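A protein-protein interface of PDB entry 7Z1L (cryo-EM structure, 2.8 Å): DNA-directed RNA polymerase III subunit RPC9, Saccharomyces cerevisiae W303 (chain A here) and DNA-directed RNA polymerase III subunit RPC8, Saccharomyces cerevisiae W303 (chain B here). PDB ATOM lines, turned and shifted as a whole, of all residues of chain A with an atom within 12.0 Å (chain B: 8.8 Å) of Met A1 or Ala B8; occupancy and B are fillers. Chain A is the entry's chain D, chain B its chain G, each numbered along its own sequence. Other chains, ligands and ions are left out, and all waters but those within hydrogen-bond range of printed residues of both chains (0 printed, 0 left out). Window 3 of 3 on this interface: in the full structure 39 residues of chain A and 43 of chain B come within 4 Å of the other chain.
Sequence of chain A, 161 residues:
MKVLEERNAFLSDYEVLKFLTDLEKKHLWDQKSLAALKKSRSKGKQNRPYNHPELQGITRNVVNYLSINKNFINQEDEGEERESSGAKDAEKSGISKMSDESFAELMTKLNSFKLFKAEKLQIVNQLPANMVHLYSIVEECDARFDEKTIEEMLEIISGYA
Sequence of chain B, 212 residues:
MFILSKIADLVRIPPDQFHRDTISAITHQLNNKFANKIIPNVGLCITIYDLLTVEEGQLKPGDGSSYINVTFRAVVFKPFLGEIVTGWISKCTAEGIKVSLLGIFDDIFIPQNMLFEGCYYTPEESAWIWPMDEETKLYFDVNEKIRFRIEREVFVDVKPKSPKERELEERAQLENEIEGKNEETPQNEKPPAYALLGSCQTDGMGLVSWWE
Among the printed residues, merely in contact across the chains: Asn A8 with Arg B73 (3.3 Å), Lys A2 with Ile B7 (3.4 Å), Met A1 with Lys B33 (3.5 Å), Met A1 with Phe B34 (3.6 Å), Met A1 with Ala B8 (3.6 Å), Val A3 with Lys B6 (3.7 Å) and Met A1 with Pro B40 (3.99 Å).
Of the printed residues of chain B, Met A1 touches Ala B8 (3.6 Å), Lys B33 (3.5 Å), Phe B34 (3.6 Å) and Pro B40 (3.99 Å). Ala B8 touches just these residues of chain A: Met A1 and Lys A2. No residue of chain A comes within 4 Å of Ile B39. No residue of chain A comes within 4 Å of Val B70. Printed residues of chain B within 4 Å of Glu A5: Lys B6 (3.4 Å). Of the printed residues of chain A, Lys B6 touches Val A3 (3.7 Å), Leu A4 (2.8 Å) and Glu A5 (3.4 Å). Of the printed residues of chain B, Val A3 touches Lys B6 (3.7 Å). Printed residues of chain A within 4 Å of Arg B73: Asn A8. Asn B69 touches none of the printed residues of chain A. Val B42 touches none of the printed residues of chain A. The nearest residue of chain A that does not touch Ala B8 is Leu A4 (4.4 Å). The nearest printed residue of chain B that does not touch Glu A5 is Ser B5 (4.1 Å).
N of Ala B8 sits at hydrogen-bond distance from O of Lys A2 (2.9 Å). N of Leu A4 sits at hydrogen-bond distance from O of Lys B6. N of Glu A5 is in hydrogen-bond range of O of Lys B6 (3.5 Å). O of Glu A6 lies within hydrogen-bond range of OG of Ser B5 (2.9 Å). The backbone carbonyl oxygen of Asn B41 lies close to the side-chain carboxylate of Glu A6 (3.0 Å).
The side-chain carboxylate (OE2) of Glu A5 lies close to the side-chain amide oxygen (OD1) of Asn A8, at 2.8 Å. N of Ile B7 sits at hydrogen-bond distance from O of Phe B72, at 2.9 Å. OD2 of Asp B9 is in salt-bridge range of NZ of Lys B33 (3.0 Å).
Of the 22 printed residues of chain B, 9 touch a printed residue of chain A. Hydrophobic or aromatic side chains of chain B within 4 Å of the printed part of chain A: Ile B7, Phe B34 and Pro B40. Among the printed residues, no Asp or Glu carboxylate lies within 4 Å of a Lys or Arg side-chain nitrogen of the other chain.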
ATOM      1  N   MET A   1      19.154   7.513   1.462  1.00  0.00           N
ATOM      2  CA  MET A   1      20.401   6.866   1.851  1.00  0.00           C
ATOM      3  C   MET A   1      20.118   5.838   2.939  1.00  0.00           C
ATOM      4  O   MET A   1      19.813   6.191   4.076  1.00  0.00           O
ATOM      5  CB  MET A   1      21.422   7.913   2.321  1.00  0.00           C
ATOM      6  CG  MET A   1      22.809   7.383   2.698  1.00  0.00           C
ATOM      7  SD  MET A   1      23.003   6.692   4.355  1.00  0.00           S
ATOM      8  CE  MET A   1      22.941   8.182   5.346  1.00  0.00           C
ATOM      9  N   LYS A   2      20.211   4.561   2.576  1.00  0.00           N
ATOM     10  CA  LYS A   2      19.982   3.461   3.500  1.00  0.00           C
ATOM     11  C   LYS A   2      21.173   2.519   3.456  1.00  0.00           C
ATOM     12  O   LYS A   2      21.612   2.120   2.372  1.00  0.00           O
ATOM     13  CB  LYS A   2      18.694   2.707   3.155  1.00  0.00           C
ATOM     14  CG  LYS A   2      18.372   1.560   4.095  1.00  0.00           C
ATOM     15  CD  LYS A   2      17.063   0.890   3.714  1.00  0.00           C
ATOM     16  CE  LYS A   2      16.660  -0.160   4.737  1.00  0.00           C
ATOM     17  NZ  LYS A   2      17.679  -1.238   4.859  1.00  0.00           N
ATOM     18  N   VAL A   3      21.694   2.166   4.626  1.00  0.00           N
ATOM     19  CA  VAL A   3      22.805   1.230   4.736  1.00  0.00           C
ATOM     20  C   VAL A   3      22.222  -0.177   4.779  1.00  0.00           C
ATOM     21  O   VAL A   3      21.618  -0.575   5.777  1.00  0.00           O
ATOM     22  CB  VAL A   3      23.664   1.514   5.972  1.00  0.00           C
ATOM     23  CG1 VAL A   3      24.925   0.669   5.945  1.00  0.00           C
ATOM     24  CG2 VAL A   3      24.012   2.991   6.047  1.00  0.00           C
ATOM     25  N   LEU A   4      22.389  -0.925   3.685  1.00  0.00           N
ATOM     26  CA  LEU A   4      21.869  -2.287   3.629  1.00  0.00           C
ATOM     27  C   LEU A   4      22.575  -3.187   4.635  1.00  0.00           C
ATOM     28  O   LEU A   4      21.937  -4.021   5.289  1.00  0.00           O
ATOM     29  CB  LEU A   4      22.012  -2.846   2.212  1.00  0.00           C
ATOM     30  CG  LEU A   4      21.092  -2.257   1.139  1.00  0.00           C
ATOM     31  CD1 LEU A   4      20.990  -3.197  -0.050  1.00  0.00           C
ATOM     32  CD2 LEU A   4      19.711  -1.956   1.701  1.00  0.00           C
ATOM     33  N   GLU A   5      23.889  -3.034   4.772  1.00  0.00           N
ATOM     34  CA  GLU A   5      24.662  -3.766   5.765  1.00  0.00           C
ATOM     35  C   GLU A   5      25.913  -2.965   6.093  1.00  0.00           C
ATOM     36  O   GLU A   5      26.584  -2.462   5.188  1.00  0.00           O
ATOM     37  CB  GLU A   5      25.015  -5.170   5.267  1.00  0.00           C
ATOM     38  CG  GLU A   5      25.502  -5.224   3.837  1.00  0.00           C
ATOM     39  CD  GLU A   5      25.641  -6.643   3.331  1.00  0.00           C
ATOM     40  OE1 GLU A   5      25.511  -7.581   4.144  1.00  0.00           O
ATOM     41  OE2 GLU A   5      25.847  -6.821   2.114  1.00  0.00           O
ATOM     42  N   GLU A   6      26.203  -2.840   7.390  1.00  0.00           N
ATOM     43  CA  GLU A   6      27.278  -1.961   7.840  1.00  0.00           C
ATOM     44  C   GLU A   6      28.640  -2.448   7.363  1.00  0.00           C
ATOM     45  O   GLU A   6      29.496  -1.642   6.981  1.00  0.00           O
ATOM     46  CB  GLU A   6      27.251  -1.847   9.364  1.00  0.00           C
ATOM     47  CG  GLU A   6      28.098  -0.720   9.921  1.00  0.00           C
ATOM     48  CD  GLU A   6      28.030  -0.636  11.433  1.00  0.00           C
ATOM     49  OE1 GLU A   6      27.383  -1.508  12.049  1.00  0.00           O
ATOM     50  OE2 GLU A   6      28.625   0.301  12.005  1.00  0.00           O
ATOM     51  N   ARG A   7      28.862  -3.760   7.375  1.00  0.00           N
ATOM     52  CA  ARG A   7      30.135  -4.343   6.966  1.00  0.00           C
ATOM     53  C   ARG A   7      29.863  -5.481   5.992  1.00  0.00           C
ATOM     54  O   ARG A   7      29.416  -6.558   6.401  1.00  0.00           O
ATOM     55  CB  ARG A   7      30.927  -4.840   8.175  1.00  0.00           C
ATOM     56  CG  ARG A   7      32.322  -5.339   7.843  1.00  0.00           C
ATOM     57  CD  ARG A   7      32.884  -6.181   8.975  1.00  0.00           C
ATOM     58  NE  ARG A   7      33.106  -5.391  10.179  1.00  0.00           N
ATOM     59  CZ  ARG A   7      32.589  -5.675  11.367  1.00  0.00           C
ATOM     60  NH1 ARG A   7      31.814  -6.732  11.547  1.00  0.00           N
ATOM     61  NH2 ARG A   7      32.855  -4.879  12.397  1.00  0.00           N
ATOM     62  N   ASN A   8      30.134  -5.244   4.710  1.00  0.00           N
ATOM     63  CA  ASN A   8      29.991  -6.280   3.694  1.00  0.00           C
ATOM     64  C   ASN A   8      31.238  -7.135   3.542  1.00  0.00           C
ATOM     65  O   ASN A   8      31.125  -8.350   3.343  1.00  0.00           O
ATOM     66  CB  ASN A   8      29.650  -5.656   2.340  1.00  0.00           C
ATOM     67  CG  ASN A   8      29.396  -6.696   1.269  1.00  0.00           C
ATOM     68  OD1 ASN A   8      28.437  -7.460   1.343  1.00  0.00           O
ATOM     69  ND2 ASN A   8      30.266  -6.738   0.269  1.00  0.00           N
ATOM     70  N   SER B   5      30.997  -1.031   2.619  1.00  0.00           N
ATOM     71  CA  SER B   5      29.615  -0.820   3.024  1.00  0.00           C
ATOM     72  C   SER B   5      28.715  -0.884   1.800  1.00  0.00           C
ATOM     73  O   SER B   5      29.025  -0.288   0.763  1.00  0.00           O
ATOM     74  CB  SER B   5      29.445   0.522   3.737  1.00  0.00           C
ATOM     75  OG  SER B   5      29.951   0.462   5.057  1.00  0.00           O
ATOM     76  N   LYS B   6      27.609  -1.614   1.928  1.00  0.00           N
ATOM     77  CA  LYS B   6      26.614  -1.739   0.872  1.00  0.00           C
ATOM     78  C   LYS B   6      25.478  -0.764   1.154  1.00  0.00           C
ATOM     79  O   LYS B   6      24.768  -0.906   2.154  1.00  0.00           O
ATOM     80  CB  LYS B   6      26.095  -3.174   0.802  1.00  0.00           C
ATOM     81  CG  LYS B   6      25.227  -3.485  -0.398  1.00  0.00           C
ATOM     82  CD  LYS B   6      25.256  -4.972  -0.703  1.00  0.00           C
ATOM     83  CE  LYS B   6      24.100  -5.380  -1.596  1.00  0.00           C
ATOM     84  NZ  LYS B   6      24.321  -6.723  -2.197  1.00  0.00           N
ATOM     85  N   ILE B   7      25.307   0.221   0.276  1.00  0.00           N
ATOM     86  CA  ILE B   7      24.389   1.328   0.502  1.00  0.00           C
ATOM     87  C   ILE B   7      23.485   1.478  -0.714  1.00  0.00           C
ATOM     88  O   ILE B   7      23.946   1.393  -1.857  1.00  0.00           O
ATOM     89  CB  ILE B   7      25.157   2.639   0.786  1.00  0.00           C
ATOM     90  CG1 ILE B   7      25.976   2.513   2.070  1.00  0.00           C
ATOM     91  CG2 ILE B   7      24.212   3.823   0.903  1.00  0.00           C
ATOM     92  CD1 ILE B   7      26.844   3.710   2.356  1.00  0.00           C
ATOM     93  N   ALA B   8      22.193   1.679  -0.466  1.00  0.00           N
ATOM     94  CA  ALA B   8      21.224   2.010  -1.501  1.00  0.00           C
ATOM     95  C   ALA B   8      20.978   3.512  -1.473  1.00  0.00           C
ATOM     96  O   ALA B   8      20.849   4.101  -0.395  1.00  0.00           O
ATOM     97  CB  ALA B   8      19.914   1.247  -1.296  1.00  0.00           C
ATOM     98  N   ASP B   9      20.913   4.125  -2.652  1.00  0.00           N
ATOM     99  CA  ASP B   9      20.864   5.575  -2.750  1.00  0.00           C
ATOM    100  C   ASP B   9      20.070   5.945  -3.995  1.00  0.00           C
ATOM    101  O   ASP B   9      19.850   5.120  -4.884  1.00  0.00           O
ATOM    102  CB  ASP B   9      22.286   6.158  -2.795  1.00  0.00           C
ATOM    103  CG  ASP B   9      22.322   7.677  -2.670  1.00  0.00           C
ATOM    104  OD1 ASP B   9      21.277   8.345  -2.804  1.00  0.00           O
ATOM    105  OD2 ASP B   9      23.426   8.210  -2.444  1.00  0.00           O
ATOM    106  N   LEU B  10      19.623   7.196  -4.035  1.00  0.00           N
ATOM    107  CA  LEU B  10      18.952   7.773  -5.191  1.00  0.00           C
ATOM    108  C   LEU B  10      19.808   8.917  -5.718  1.00  0.00           C
ATOM    109  O   LEU B  10      19.970   9.936  -5.039  1.00  0.00           O
ATOM    110  CB  LEU B  10      17.555   8.268  -4.816  1.00  0.00           C
ATOM    111  CG  LEU B  10      16.696   8.873  -5.924  1.00  0.00           C
ATOM    112  CD1 LEU B  10      16.075   7.783  -6.778  1.00  0.00           C
ATOM    113  CD2 LEU B  10      15.627   9.764  -5.324  1.00  0.00           C
ATOM    114  N   VAL B  11      20.352   8.749  -6.920  1.00  0.00           N
ATOM    115  CA  VAL B  11      21.278   9.711  -7.508  1.00  0.00           C
ATOM    116  C   VAL B  11      20.585  10.439  -8.649  1.00  0.00           C
ATOM    117  O   VAL B  11      19.840   9.838  -9.430  1.00  0.00           O
ATOM    118  CB  VAL B  11      22.576   9.038  -7.993  1.00  0.00           C
ATOM    119  CG1 VAL B  11      23.437   8.658  -6.808  1.00  0.00           C
ATOM    120  CG2 VAL B  11      22.269   7.813  -8.834  1.00  0.00           C
ATOM    121  N   LEU B  30      27.819   9.965  -6.846  1.00  0.00           N
ATOM    122  CA  LEU B  30      28.053   9.330  -5.554  1.00  0.00           C
ATOM    123  C   LEU B  30      29.318   9.863  -4.894  1.00  0.00           C
ATOM    124  O   LEU B  30      29.375   9.983  -3.667  1.00  0.00           O
ATOM    125  CB  LEU B  30      28.125   7.815  -5.724  1.00  0.00           C
ATOM    126  CG  LEU B  30      26.795   7.107  -5.959  1.00  0.00           C
ATOM    127  CD1 LEU B  30      27.027   5.719  -6.521  1.00  0.00           C
ATOM    128  CD2 LEU B  30      25.998   7.046  -4.672  1.00  0.00           C
ATOM    129  N   LYS B  33      28.456  13.106  -3.356  1.00  0.00           N
ATOM    130  CA  LYS B  33      27.652  12.985  -2.144  1.00  0.00           C
ATOM    131  C   LYS B  33      28.435  12.405  -0.967  1.00  0.00           C
ATOM    132  O   LYS B  33      28.229  12.823   0.177  1.00  0.00           O
ATOM    133  CB  LYS B  33      26.415  12.132  -2.417  1.00  0.00           C
ATOM    134  CG  LYS B  33      25.333  12.278  -1.362  1.00  0.00           C
ATOM    135  CD  LYS B  33      24.336  11.142  -1.432  1.00  0.00           C
ATOM    136  CE  LYS B  33      23.295  11.257  -0.334  1.00  0.00           C
ATOM    137  NZ  LYS B  33      22.428  10.050  -0.263  1.00  0.00           N
ATOM    138  N   PHE B  34      29.338  11.454  -1.217  1.00  0.00           N
ATOM    139  CA  PHE B  34      29.839  10.573  -0.167  1.00  0.00           C
ATOM    140  C   PHE B  34      31.321  10.709   0.149  1.00  0.00           C
ATOM    141  O   PHE B  34      31.719  10.377   1.268  1.00  0.00           O
ATOM    142  CB  PHE B  34      29.566   9.108  -0.535  1.00  0.00           C
ATOM    143  CG  PHE B  34      28.216   8.618  -0.113  1.00  0.00           C
ATOM    144  CD1 PHE B  34      27.926   8.413   1.223  1.00  0.00           C
ATOM    145  CD2 PHE B  34      27.234   8.366  -1.052  1.00  0.00           C
ATOM    146  CE1 PHE B  34      26.684   7.964   1.614  1.00  0.00           C
ATOM    147  CE2 PHE B  34      25.991   7.917  -0.666  1.00  0.00           C
ATOM    148  CZ  PHE B  34      25.716   7.715   0.667  1.00  0.00           C
ATOM    149  N   ILE B  38      31.257  11.761   6.587  1.00  0.00           N
ATOM    150  CA  ILE B  38      30.914  10.819   7.645  1.00  0.00           C
ATOM    151  C   ILE B  38      29.555  10.208   7.329  1.00  0.00           C
ATOM    152  O   ILE B  38      28.532  10.898   7.344  1.00  0.00           O
ATOM    153  CB  ILE B  38      30.904  11.498   9.019  1.00  0.00           C
ATOM    154  CG1 ILE B  38      32.297  12.022   9.371  1.00  0.00           C
ATOM    155  CG2 ILE B  38      30.412  10.534  10.085  1.00  0.00           C
ATOM    156  CD1 ILE B  38      33.333  10.937   9.531  1.00  0.00           C
ATOM    157  N   ILE B  39      29.545   8.913   7.040  1.00  0.00           N
ATOM    158  CA  ILE B  39      28.304   8.148   7.003  1.00  0.00           C
ATOM    159  C   ILE B  39      27.921   7.886   8.454  1.00  0.00           C
ATOM    160  O   ILE B  39      28.710   7.276   9.197  1.00  0.00           O
ATOM    161  CB  ILE B  39      28.458   6.841   6.212  1.00  0.00           C
ATOM    162  CG1 ILE B  39      29.012   7.122   4.819  1.00  0.00           C
ATOM    163  CG2 ILE B  39      27.123   6.129   6.104  1.00  0.00           C
ATOM    164  CD1 ILE B  39      29.350   5.873   4.048  1.00  0.00           C
ATOM    165  N   PRO B  40      26.744   8.334   8.895  1.00  0.00           N
ATOM    166  CA  PRO B  40      26.403   8.259  10.321  1.00  0.00           C
ATOM    167  C   PRO B  40      26.296   6.822  10.808  1.00  0.00           C
ATOM    168  O   PRO B  40      25.745   5.955  10.127  1.00  0.00           O
ATOM    169  CB  PRO B  40      25.052   8.980  10.401  1.00  0.00           C
ATOM    170  CG  PRO B  40      24.971   9.797   9.151  1.00  0.00           C
ATOM    171  CD  PRO B  40      25.694   9.003   8.113  1.00  0.00           C
ATOM    172  N   ASN B  41      26.853   6.585  11.998  1.00  0.00           N
ATOM    173  CA  ASN B  41      26.924   5.272  12.641  1.00  0.00           C
ATOM    174  C   ASN B  41      27.653   4.238  11.784  1.00  0.00           C
ATOM    175  O   ASN B  41      27.497   3.032  11.998  1.00  0.00           O
ATOM    176  CB  ASN B  41      25.531   4.758  13.024  1.00  0.00           C
ATOM    177  CG  ASN B  41      24.852   5.637  14.056  1.00  0.00           C
ATOM    178  OD1 ASN B  41      23.831   6.266  13.779  1.00  0.00           O
ATOM    179  ND2 ASN B  41      25.419   5.687  15.255  1.00  0.00           N
ATOM    180  N   VAL B  42      28.450   4.685  10.815  1.00  0.00           N
ATOM    181  CA  VAL B  42      29.220   3.783   9.967  1.00  0.00           C
ATOM    182  C   VAL B  42      30.687   4.185  10.004  1.00  0.00           C
ATOM    183  O   VAL B  42      31.553   3.370  10.337  1.00  0.00           O
ATOM    184  CB  VAL B  42      28.686   3.771   8.524  1.00  0.00           C
ATOM    185  CG1 VAL B  42      29.642   3.019   7.614  1.00  0.00           C
ATOM    186  CG2 VAL B  42      27.303   3.144   8.475  1.00  0.00           C
ATOM    187  N   THR B  53      23.710  -2.975  -8.448  1.00  0.00           N
ATOM    188  CA  THR B  53      22.472  -2.909  -9.212  1.00  0.00           C
ATOM    189  C   THR B  53      22.129  -1.456  -9.500  1.00  0.00           C
ATOM    190  O   THR B  53      22.345  -0.581  -8.659  1.00  0.00           O
ATOM    191  CB  THR B  53      21.295  -3.568  -8.472  1.00  0.00           C
ATOM    192  OG1 THR B  53      21.058  -2.882  -7.236  1.00  0.00           O
ATOM    193  CG2 THR B  53      21.568  -5.042  -8.194  1.00  0.00           C
ATOM    194  N   ILE B  68      18.052   7.806 -10.461  1.00  0.00           N
ATOM    195  CA  ILE B  68      18.362   6.384 -10.530  1.00  0.00           C
ATOM    196  C   ILE B  68      18.531   5.850  -9.116  1.00  0.00           C
ATOM    197  O   ILE B  68      19.249   6.444  -8.304  1.00  0.00           O
ATOM    198  CB  ILE B  68      19.630   6.115 -11.361  1.00  0.00           C
ATOM    199  CG1 ILE B  68      19.584   6.891 -12.679  1.00  0.00           C
ATOM    200  CG2 ILE B  68      19.795   4.627 -11.608  1.00  0.00           C
ATOM    201  CD1 ILE B  68      20.649   6.485 -13.670  1.00  0.00           C
ATOM    202  N   ASN B  69      17.866   4.736  -8.824  1.00  0.00           N
ATOM    203  CA  ASN B  69      18.088   4.000  -7.588  1.00  0.00           C
ATOM    204  C   ASN B  69      19.256   3.048  -7.803  1.00  0.00           C
ATOM    205  O   ASN B  69      19.207   2.191  -8.691  1.00  0.00           O
ATOM    206  CB  ASN B  69      16.831   3.236  -7.178  1.00  0.00           C
ATOM    207  CG  ASN B  69      15.894   4.070  -6.332  1.00  0.00           C
ATOM    208  OD1 ASN B  69      16.294   4.644  -5.321  1.00  0.00           O
ATOM    209  ND2 ASN B  69      14.638   4.152  -6.750  1.00  0.00           N
ATOM    210  N   VAL B  70      20.304   3.198  -6.997  1.00  0.00           N
ATOM    211  CA  VAL B  70      21.558   2.484  -7.197  1.00  0.00           C
ATOM    212  C   VAL B  70      21.994   1.857  -5.877  1.00  0.00           C
ATOM    213  O   VAL B  70      21.875   2.475  -4.815  1.00  0.00           O
ATOM    214  CB  VAL B  70      22.648   3.412  -7.776  1.00  0.00           C
ATOM    215  CG1 VAL B  70      22.949   4.577  -6.844  1.00  0.00           C
ATOM    216  CG2 VAL B  70      23.918   2.636  -8.079  1.00  0.00           C
ATOM    217  N   THR B  71      22.457   0.613  -5.943  1.00  0.00           N
ATOM    218  CA  THR B  71      23.088  -0.055  -4.813  1.00  0.00           C
ATOM    219  C   THR B  71      24.581  -0.147  -5.089  1.00  0.00           C
ATOM    220  O   THR B  71      24.991  -0.584  -6.168  1.00  0.00           O
ATOM    221  CB  THR B  71      22.496  -1.447  -4.591  1.00  0.00           C
ATOM    222  OG1 THR B  71      21.094  -1.334  -4.325  1.00  0.00           O
ATOM    223  CG2 THR B  71      23.174  -2.137  -3.419  1.00  0.00           C
ATOM    224  N   PHE B  72      25.392   0.276  -4.124  1.00  0.00           N
ATOM    225  CA  PHE B  72      26.822   0.381  -4.361  1.00  0.00           C
ATOM    226  C   PHE B  72      27.589  -0.050  -3.121  1.00  0.00           C
ATOM    227  O   PHE B  72      27.105   0.048  -1.991  1.00  0.00           O
ATOM    228  CB  PHE B  72      27.216   1.806  -4.773  1.00  0.00           C
ATOM    229  CG  PHE B  72      27.051   2.829  -3.684  1.00  0.00           C
ATOM    230  CD1 PHE B  72      25.809   3.364  -3.401  1.00  0.00           C
ATOM    231  CD2 PHE B  72      28.139   3.258  -2.945  1.00  0.00           C
ATOM    232  CE1 PHE B  72      25.654   4.301  -2.404  1.00  0.00           C
ATOM    233  CE2 PHE B  72      27.991   4.195  -1.947  1.00  0.00           C
ATOM    234  CZ  PHE B  72      26.748   4.717  -1.677  1.00  0.00           C
ATOM    235  N   ARG B  73      28.811  -0.518  -3.353  1.00  0.00           N
ATOM    236  CA  ARG B  73      29.760  -0.824  -2.292  1.00  0.00           C
ATOM    237  C   ARG B  73      30.792   0.291  -2.254  1.00  0.00           C
ATOM    238  O   ARG B  73      31.362   0.651  -3.295  1.00  0.00           O
ATOM    239  CB  ARG B  73      30.438  -2.173  -2.521  1.00  0.00           C
ATOM    240  CG  ARG B  73      29.495  -3.354  -2.551  1.00  0.00           C
ATOM    241  CD  ARG B  73      30.254  -4.643  -2.308  1.00  0.00           C
ATOM    242  NE  ARG B  73      31.203  -4.925  -3.377  1.00  0.00           N
ATOM    243  CZ  ARG B  73      31.442  -6.134  -3.865  1.00  0.00           C
ATOM    244  NH1 ARG B  73      30.817  -7.204  -3.400  1.00  0.00           N
ATOM    245  NH2 ARG B  73      32.333  -6.274  -4.843  1.00  0.00           N
